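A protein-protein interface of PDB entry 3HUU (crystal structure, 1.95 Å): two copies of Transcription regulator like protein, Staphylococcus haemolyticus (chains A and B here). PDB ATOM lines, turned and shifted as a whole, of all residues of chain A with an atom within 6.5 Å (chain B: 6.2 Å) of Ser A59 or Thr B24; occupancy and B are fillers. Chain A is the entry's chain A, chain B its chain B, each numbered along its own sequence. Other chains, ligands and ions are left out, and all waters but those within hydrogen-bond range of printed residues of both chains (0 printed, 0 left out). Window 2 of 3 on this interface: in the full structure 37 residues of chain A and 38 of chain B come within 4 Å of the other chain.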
ATOM      1  N   THR A  22       2.823 -25.791  29.192  1.00  0.00           N
ATOM      2  CA  THR A  22       3.873 -24.998  28.566  1.00  0.00           C
ATOM      3  C   THR A  22       3.352 -24.397  27.264  1.00  0.00           C
ATOM      4  O   THR A  22       3.920 -23.442  26.734  1.00  0.00           O
ATOM      5  CB  THR A  22       5.106 -25.868  28.238  1.00  0.00           C
ATOM      6  OG1 THR A  22       4.775 -26.788  27.190  1.00  0.00           O
ATOM      7  CG2 THR A  22       5.544 -26.662  29.469  1.00  0.00           C
ATOM      8  N   LEU A  23       2.255 -24.960  26.766  1.00  0.00           N
ATOM      9  CA  LEU A  23       1.664 -24.521  25.508  1.00  0.00           C
ATOM     10  C   LEU A  23       2.731 -24.588  24.420  1.00  0.00           C
ATOM     11  O   LEU A  23       2.773 -23.756  23.511  1.00  0.00           O
ATOM     12  CB  LEU A  23       1.122 -23.095  25.630  1.00  0.00           C
ATOM     13  CG  LEU A  23      -0.101 -22.922  26.545  1.00  0.00           C
ATOM     14  CD1 LEU A  23      -0.529 -21.458  26.554  1.00  0.00           C
ATOM     15  CD2 LEU A  23      -1.242 -23.808  26.056  1.00  0.00           C
ATOM     16  N   THR A  24       3.599 -25.590  24.532  1.00  0.00           N
ATOM     17  CA  THR A  24       4.668 -25.791  23.570  1.00  0.00           C
ATOM     18  C   THR A  24       4.596 -27.206  23.013  1.00  0.00           C
ATOM     19  O   THR A  24       4.165 -28.143  23.703  1.00  0.00           O
ATOM     20  CB  THR A  24       6.051 -25.585  24.217  1.00  0.00           C
ATOM     21  OG1 THR A  24       6.103 -24.293  24.833  1.00  0.00           O
ATOM     22  CG2 THR A  24       7.149 -25.673  23.170  1.00  0.00           C
ATOM     23  N   ILE A  25       5.011 -27.357  21.760  1.00  0.00           N
ATOM     24  CA  ILE A  25       5.002 -28.661  21.112  1.00  0.00           C
ATOM     25  C   ILE A  25       6.438 -29.009  20.759  1.00  0.00           C
ATOM     26  O   ILE A  25       7.152 -28.200  20.177  1.00  0.00           O
ATOM     27  CB  ILE A  25       4.161 -28.645  19.822  1.00  0.00           C
ATOM     28  CG1 ILE A  25       2.740 -28.170  20.136  1.00  0.00           C
ATOM     29  CG2 ILE A  25       4.101 -30.050  19.214  1.00  0.00           C
ATOM     30  CD1 ILE A  25       1.949 -29.114  21.038  1.00  0.00           C
ATOM     31  N   GLY A  26       6.864 -30.212  21.132  1.00  0.00           N
ATOM     32  CA  GLY A  26       8.218 -30.629  20.829  1.00  0.00           C
ATOM     33  C   GLY A  26       8.244 -31.294  19.467  1.00  0.00           C
ATOM     34  O   GLY A  26       7.439 -32.194  19.195  1.00  0.00           O
ATOM     35  N   CYS A  53      -0.006 -23.924  14.960  1.00  0.00           N
ATOM     36  CA  CYS A  53       0.294 -23.501  16.320  1.00  0.00           C
ATOM     37  C   CYS A  53       0.152 -22.000  16.610  1.00  0.00           C
ATOM     38  O   CYS A  53      -0.360 -21.615  17.668  1.00  0.00           O
ATOM     39  CB  CYS A  53       1.695 -23.979  16.698  1.00  0.00           C
ATOM     40  SG  CYS A  53       1.852 -25.796  16.645  1.00  0.00           S
ATOM     41  N   ASN A  54       0.604 -21.154  15.690  1.00  0.00           N
ATOM     42  CA  ASN A  54       0.514 -19.710  15.896  1.00  0.00           C
ATOM     43  C   ASN A  54      -0.923 -19.220  16.060  1.00  0.00           C
ATOM     44  O   ASN A  54      -1.197 -18.362  16.896  1.00  0.00           O
ATOM     45  CB  ASN A  54       1.207 -18.968  14.748  1.00  0.00           C
ATOM     46  CG  ASN A  54       2.735 -18.942  14.897  1.00  0.00           C
ATOM     47  OD1 ASN A  54       3.317 -19.750  15.626  1.00  0.00           O
ATOM     48  ND2 ASN A  54       3.383 -18.020  14.194  1.00  0.00           N
ATOM     49  N   GLY A  57      -2.261 -20.457  19.574  1.00  0.00           N
ATOM     50  CA  GLY A  57      -1.502 -20.088  20.754  1.00  0.00           C
ATOM     51  C   GLY A  57      -0.499 -21.080  21.317  1.00  0.00           C
ATOM     52  O   GLY A  57      -0.391 -21.216  22.536  1.00  0.00           O
ATOM     53  N   TYR A  58       0.239 -21.771  20.452  1.00  0.00           N
ATOM     54  CA  TYR A  58       1.250 -22.720  20.911  1.00  0.00           C
ATOM     55  C   TYR A  58       2.638 -22.313  20.421  1.00  0.00           C
ATOM     56  O   TYR A  58       2.776 -21.716  19.354  1.00  0.00           O
ATOM     57  CB  TYR A  58       0.931 -24.138  20.421  1.00  0.00           C
ATOM     58  CG  TYR A  58       0.000 -24.901  21.331  1.00  0.00           C
ATOM     59  CD1 TYR A  58      -1.361 -24.614  21.375  1.00  0.00           C
ATOM     60  CD2 TYR A  58       0.492 -25.884  22.187  1.00  0.00           C
ATOM     61  CE1 TYR A  58      -2.213 -25.292  22.258  1.00  0.00           C
ATOM     62  CE2 TYR A  58      -0.344 -26.564  23.069  1.00  0.00           C
ATOM     63  CZ  TYR A  58      -1.696 -26.263  23.101  1.00  0.00           C
ATOM     64  OH  TYR A  58      -2.518 -26.928  23.980  1.00  0.00           O
ATOM     65  N   SER A  59       3.660 -22.618  21.219  1.00  0.00           N
ATOM     66  CA  SER A  59       5.044 -22.309  20.865  1.00  0.00           C
ATOM     67  C   SER A  59       5.673 -23.583  20.320  1.00  0.00           C
ATOM     68  O   SER A  59       5.026 -24.626  20.275  1.00  0.00           O
ATOM     69  CB  SER A  59       5.830 -21.843  22.090  1.00  0.00           C
ATOM     70  OG  SER A  59       5.301 -20.641  22.624  1.00  0.00           O
ATOM     71  N   THR A  60       6.940 -23.509  19.933  1.00  0.00           N
ATOM     72  CA  THR A  60       7.607 -24.682  19.394  1.00  0.00           C
ATOM     73  C   THR A  60       9.057 -24.842  19.829  1.00  0.00           C
ATOM     74  O   THR A  60       9.757 -23.867  20.097  1.00  0.00           O
ATOM     75  CB  THR A  60       7.509 -24.682  17.844  1.00  0.00           C
ATOM     76  OG1 THR A  60       6.262 -25.272  17.453  1.00  0.00           O
ATOM     77  CG2 THR A  60       8.652 -25.453  17.221  1.00  0.00           C
ATOM     78  N   ARG A  61       9.484 -26.098  19.921  1.00  0.00           N
ATOM     79  CA  ARG A  61      10.848 -26.444  20.290  1.00  0.00           C
ATOM     80  C   ARG A  61      11.246 -27.624  19.410  1.00  0.00           C
ATOM     81  O   ARG A  61      10.522 -28.624  19.334  1.00  0.00           O
ATOM     82  CB  ARG A  61      10.914 -26.838  21.768  1.00  0.00           C
ATOM     83  CG  ARG A  61      10.678 -25.672  22.722  1.00  0.00           C
ATOM     84  CD  ARG A  61      11.987 -25.002  23.106  1.00  0.00           C
ATOM     85  NE  ARG A  61      12.600 -25.641  24.269  1.00  0.00           N
ATOM     86  CZ  ARG A  61      12.109 -25.568  25.503  1.00  0.00           C
ATOM     87  NH1 ARG A  61      10.998 -24.879  25.733  1.00  0.00           N
ATOM     88  NH2 ARG A  61      12.725 -26.186  26.506  1.00  0.00           N
ATOM     89  N   THR B  24       9.956 -17.045  25.054  1.00  0.00           N
ATOM     90  CA  THR B  24       9.776 -17.289  23.595  1.00  0.00           C
ATOM     91  C   THR B  24      10.415 -16.174  22.776  1.00  0.00           C
ATOM     92  O   THR B  24      10.220 -14.988  23.063  1.00  0.00           O
ATOM     93  CB  THR B  24       8.279 -17.368  23.226  1.00  0.00           C
ATOM     94  OG1 THR B  24       7.644 -18.390  24.008  1.00  0.00           O
ATOM     95  CG2 THR B  24       8.110 -17.697  21.747  1.00  0.00           C
ATOM     96  N   ILE B  25      11.191 -16.553  21.764  1.00  0.00           N
ATOM     97  CA  ILE B  25      11.833 -15.571  20.896  1.00  0.00           C
ATOM     98  C   ILE B  25      11.161 -15.635  19.535  1.00  0.00           C
ATOM     99  O   ILE B  25      10.928 -16.720  19.001  1.00  0.00           O
ATOM    100  CB  ILE B  25      13.340 -15.853  20.715  1.00  0.00           C
ATOM    101  CG1 ILE B  25      14.058 -15.737  22.059  1.00  0.00           C
ATOM    102  CG2 ILE B  25      13.941 -14.853  19.732  1.00  0.00           C
ATOM    103  CD1 ILE B  25      13.995 -14.365  22.663  1.00  0.00           C
ATOM    104  N   GLY B  26      10.838 -14.471  18.984  1.00  0.00           N
ATOM    105  CA  GLY B  26      10.199 -14.441  17.687  1.00  0.00           C
ATOM    106  C   GLY B  26      11.242 -14.372  16.590  1.00  0.00           C
ATOM    107  O   GLY B  26      12.189 -13.595  16.675  1.00  0.00           O
ATOM    108  N   TYR B  58      14.436 -21.580  26.458  1.00  0.00           N
ATOM    109  CA  TYR B  58      13.631 -20.678  25.641  1.00  0.00           C
ATOM    110  C   TYR B  58      13.001 -21.433  24.477  1.00  0.00           C
ATOM    111  O   TYR B  58      13.628 -22.314  23.893  1.00  0.00           O
ATOM    112  CB  TYR B  58      14.497 -19.542  25.093  1.00  0.00           C
ATOM    113  CG  TYR B  58      14.622 -18.357  26.019  1.00  0.00           C
ATOM    114  CD1 TYR B  58      13.629 -17.385  26.071  1.00  0.00           C
ATOM    115  CD2 TYR B  58      15.741 -18.198  26.831  1.00  0.00           C
ATOM    116  CE1 TYR B  58      13.750 -16.274  26.910  1.00  0.00           C
ATOM    117  CE2 TYR B  58      15.872 -17.097  27.670  1.00  0.00           C
ATOM    118  CZ  TYR B  58      14.873 -16.137  27.704  1.00  0.00           C
ATOM    119  OH  TYR B  58      15.003 -15.044  28.531  1.00  0.00           O
ATOM    120  N   SER B  59      11.751 -21.111  24.166  1.00  0.00           N
ATOM    121  CA  SER B  59      11.085 -21.752  23.048  1.00  0.00           C
ATOM    122  C   SER B  59      11.213 -20.748  21.910  1.00  0.00           C
ATOM    123  O   SER B  59      11.821 -19.683  22.074  1.00  0.00           O
ATOM    124  CB  SER B  59       9.611 -22.040  23.362  1.00  0.00           C
ATOM    125  OG  SER B  59       8.825 -20.866  23.303  1.00  0.00           O
ATOM    126  N   THR B  60      10.652 -21.066  20.756  1.00  0.00           N
ATOM    127  CA  THR B  60      10.773 -20.141  19.650  1.00  0.00           C
ATOM    128  C   THR B  60       9.493 -20.090  18.843  1.00  0.00           C
ATOM    129  O   THR B  60       8.662 -21.002  18.904  1.00  0.00           O
ATOM    130  CB  THR B  60      11.961 -20.539  18.743  1.00  0.00           C
ATOM    131  OG1 THR B  60      12.378 -19.409  17.971  1.00  0.00           O
ATOM    132  CG2 THR B  60      11.560 -21.673  17.810  1.00  0.00           C
ATOM    133  N   ARG B  61       9.332 -19.002  18.103  1.00  0.00           N
ATOM    134  CA  ARG B  61       8.165 -18.804  17.270  1.00  0.00           C
ATOM    135  C   ARG B  61       8.631 -18.155  15.975  1.00  0.00           C
ATOM    136  O   ARG B  61       9.398 -17.202  15.999  1.00  0.00           O
ATOM    137  CB  ARG B  61       7.164 -17.891  17.975  1.00  0.00           C
ATOM    138  CG  ARG B  61       5.894 -17.635  17.175  1.00  0.00           C
ATOM    139  CD  ARG B  61       5.037 -16.568  17.837  1.00  0.00           C
ATOM    140  NE  ARG B  61       4.718 -16.914  19.217  1.00  0.00           N
ATOM    141  CZ  ARG B  61       3.999 -17.972  19.578  1.00  0.00           C
ATOM    142  NH1 ARG B  61       3.515 -18.795  18.655  1.00  0.00           N
ATOM    143  NH2 ARG B  61       3.763 -18.209  20.863  1.00  0.00           N
ATOM    144  N   SER B  83       2.864 -12.611  22.796  1.00  0.00           N
ATOM    145  CA  SER B  83       3.154 -14.032  22.650  1.00  0.00           C
ATOM    146  C   SER B  83       4.655 -14.263  22.505  1.00  0.00           C
ATOM    147  O   SER B  83       5.103 -15.399  22.330  1.00  0.00           O
ATOM    148  CB  SER B  83       2.415 -14.607  21.432  1.00  0.00           C
ATOM    149  OG  SER B  83       2.886 -14.044  20.217  1.00  0.00           O
ATOM    150  N   VAL B  84       5.430 -13.185  22.593  1.00  0.00           N
ATOM    151  CA  VAL B  84       6.882 -13.269  22.466  1.00  0.00           C
ATOM    152  C   VAL B  84       7.567 -12.265  23.393  1.00  0.00           C
ATOM    153  O   VAL B  84       6.983 -11.239  23.729  1.00  0.00           O
ATOM    154  CB  VAL B  84       7.330 -12.974  21.013  1.00  0.00           C
ATOM    155  CG1 VAL B  84       8.814 -13.239  20.866  1.00  0.00           C
ATOM    156  CG2 VAL B  84       6.532 -13.824  20.032  1.00  0.00           C
ATOM    157  N   ASP B  85       8.802 -12.563  23.794  1.00  0.00           N
ATOM    158  CA  ASP B  85       9.575 -11.685  24.677  1.00  0.00           C
ATOM    159  C   ASP B  85      10.570 -10.812  23.918  1.00  0.00           C
ATOM    160  O   ASP B  85      10.935  -9.732  24.377  1.00  0.00           O
ATOM    161  CB  ASP B  85      10.350 -12.509  25.709  1.00  0.00           C
ATOM    162  CG  ASP B  85       9.462 -13.067  26.805  1.00  0.00           C
ATOM    163  OD1 ASP B  85       9.964 -13.876  27.618  1.00  0.00           O
ATOM    164  OD2 ASP B  85       8.273 -12.696  26.861  1.00  0.00           O
ATOM    165  N   GLY B  86      11.022 -11.300  22.764  1.00  0.00           N
ATOM    166  CA  GLY B  86      11.973 -10.556  21.956  1.00  0.00           C
ATOM    167  C   GLY B  86      11.990 -11.111  20.543  1.00  0.00           C
ATOM    168  O   GLY B  86      11.421 -12.175  20.293  1.00  0.00           O
ATOM    169  N   LEU B 272      17.485  -9.765  26.865  1.00  0.00           N
ATOM    170  CA  LEU B 272      16.305  -9.914  27.711  1.00  0.00           C
ATOM    171  C   LEU B 272      16.712 -10.165  29.166  1.00  0.00           C
ATOM    172  O   LEU B 272      16.892 -11.308  29.583  1.00  0.00           O
ATOM    173  CB  LEU B 272      15.433 -11.066  27.202  1.00  0.00           C
ATOM    174  CG  LEU B 272      14.854 -10.930  25.789  1.00  0.00           C
ATOM    175  CD1 LEU B 272      14.184 -12.237  25.401  1.00  0.00           C
ATOM    176  CD2 LEU B 272      13.861  -9.769  25.729  1.00  0.00           C
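The guanidinium group (NH1) of Arg B61 is in hydrogen-bond range of the side-chain amide oxygen (OD1) of Asn A54.
The guanidinium group (NH1) of Arg B61 lies within hydrogen-bond range of the backbone carbonyl oxygen (O) of Tyr A58, 3.1 Å away.
The side-chain hydroxyl (OG) of Ser A59 is in hydrogen-bond range of the guanidinium group (NH2) of Arg B61 (3.4 Å).
The backbone carbonyl oxygen (O) of Thr A60 is in hydrogen-bond range of the backbone NH (N) of Thr B60 (3.0 Å).
The backbone NH (N) of Ser A59 sits at hydrogen-bond distance from the backbone carbonyl oxygen (O) of Leu A23, 2.7 Å away.
The side-chain hydroxyl of Thr B24 sits at hydrogen-bond distance from the side-chain hydroxyl of Ser B59 (2.8 Å).
The backbone NH (N) of Asp B85 lies within hydrogen-bond range of the backbone carbonyl oxygen (O) of Thr B24, at 2.9 Å.
The backbone NH of Ile B25 sits at hydrogen-bond distance from the backbone carbonyl oxygen of Ser B59, at 3.2 Å.
OG1 of Thr B60 sits at hydrogen-bond distance from O of Ile B25 (3.2 Å).
The backbone carbonyl oxygen of Ile B25 lies within hydrogen-bond range of the backbone NH of Arg B61 (2.9 Å).
Among the printed residues, merely in contact across the chains: Arg A61 with Tyr B58, Arg A61 with Ser B59, Ser A59 with Ser B59, Ser A59 with Thr B24 and Thr A60 with Ser B59.
Of chain B, only Thr B24 (3.5 Å), Ser B59 (3.4 Å) and Arg B61 (3.4 Å) come within 4 Å of Ser A59.
Of the printed residues of chain A, Tyr B58 touches Arg A61 (3.2 Å).
Of the printed residues of chain A, Arg B61 touches Asn A54, Tyr A58 and Ser A59.
Printed residues of chain B within 4 Å of Asn A54: Arg B61.
Leu B272 touches none of the printed residues of chain A.
The nearest residue of chain B that does not touch Ser A59 is Thr B60 (4.2 Å).
The nearest residue of chain A that does not touch Thr B24 is Thr A24 (6.2 Å).
The nearest printed residue of chain A that does not touch Tyr B58 is Thr A60 (5.6 Å).
Of the 12 printed residues of chain B, 5 touch a printed residue of chain A.
Among the printed residues, 9 pairs touch across the chains.
Tyr A58 touches Arg B61, and with the chains exchanged Arg A61 touches Tyr B58.
Ser A59 touches Thr B24, but with the chains exchanged Thr A24 does not touch Ser B59 (4.4 Å).
Ser A59 touches Arg B61, and with the chains exchanged Arg A61 touches Ser B59.
Thr B60 touches its own counterpart, Thr A60.
Of the 9 pairs that touch across the chains among the printed residues, 6 have their exchanged pair printed and touching as well.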
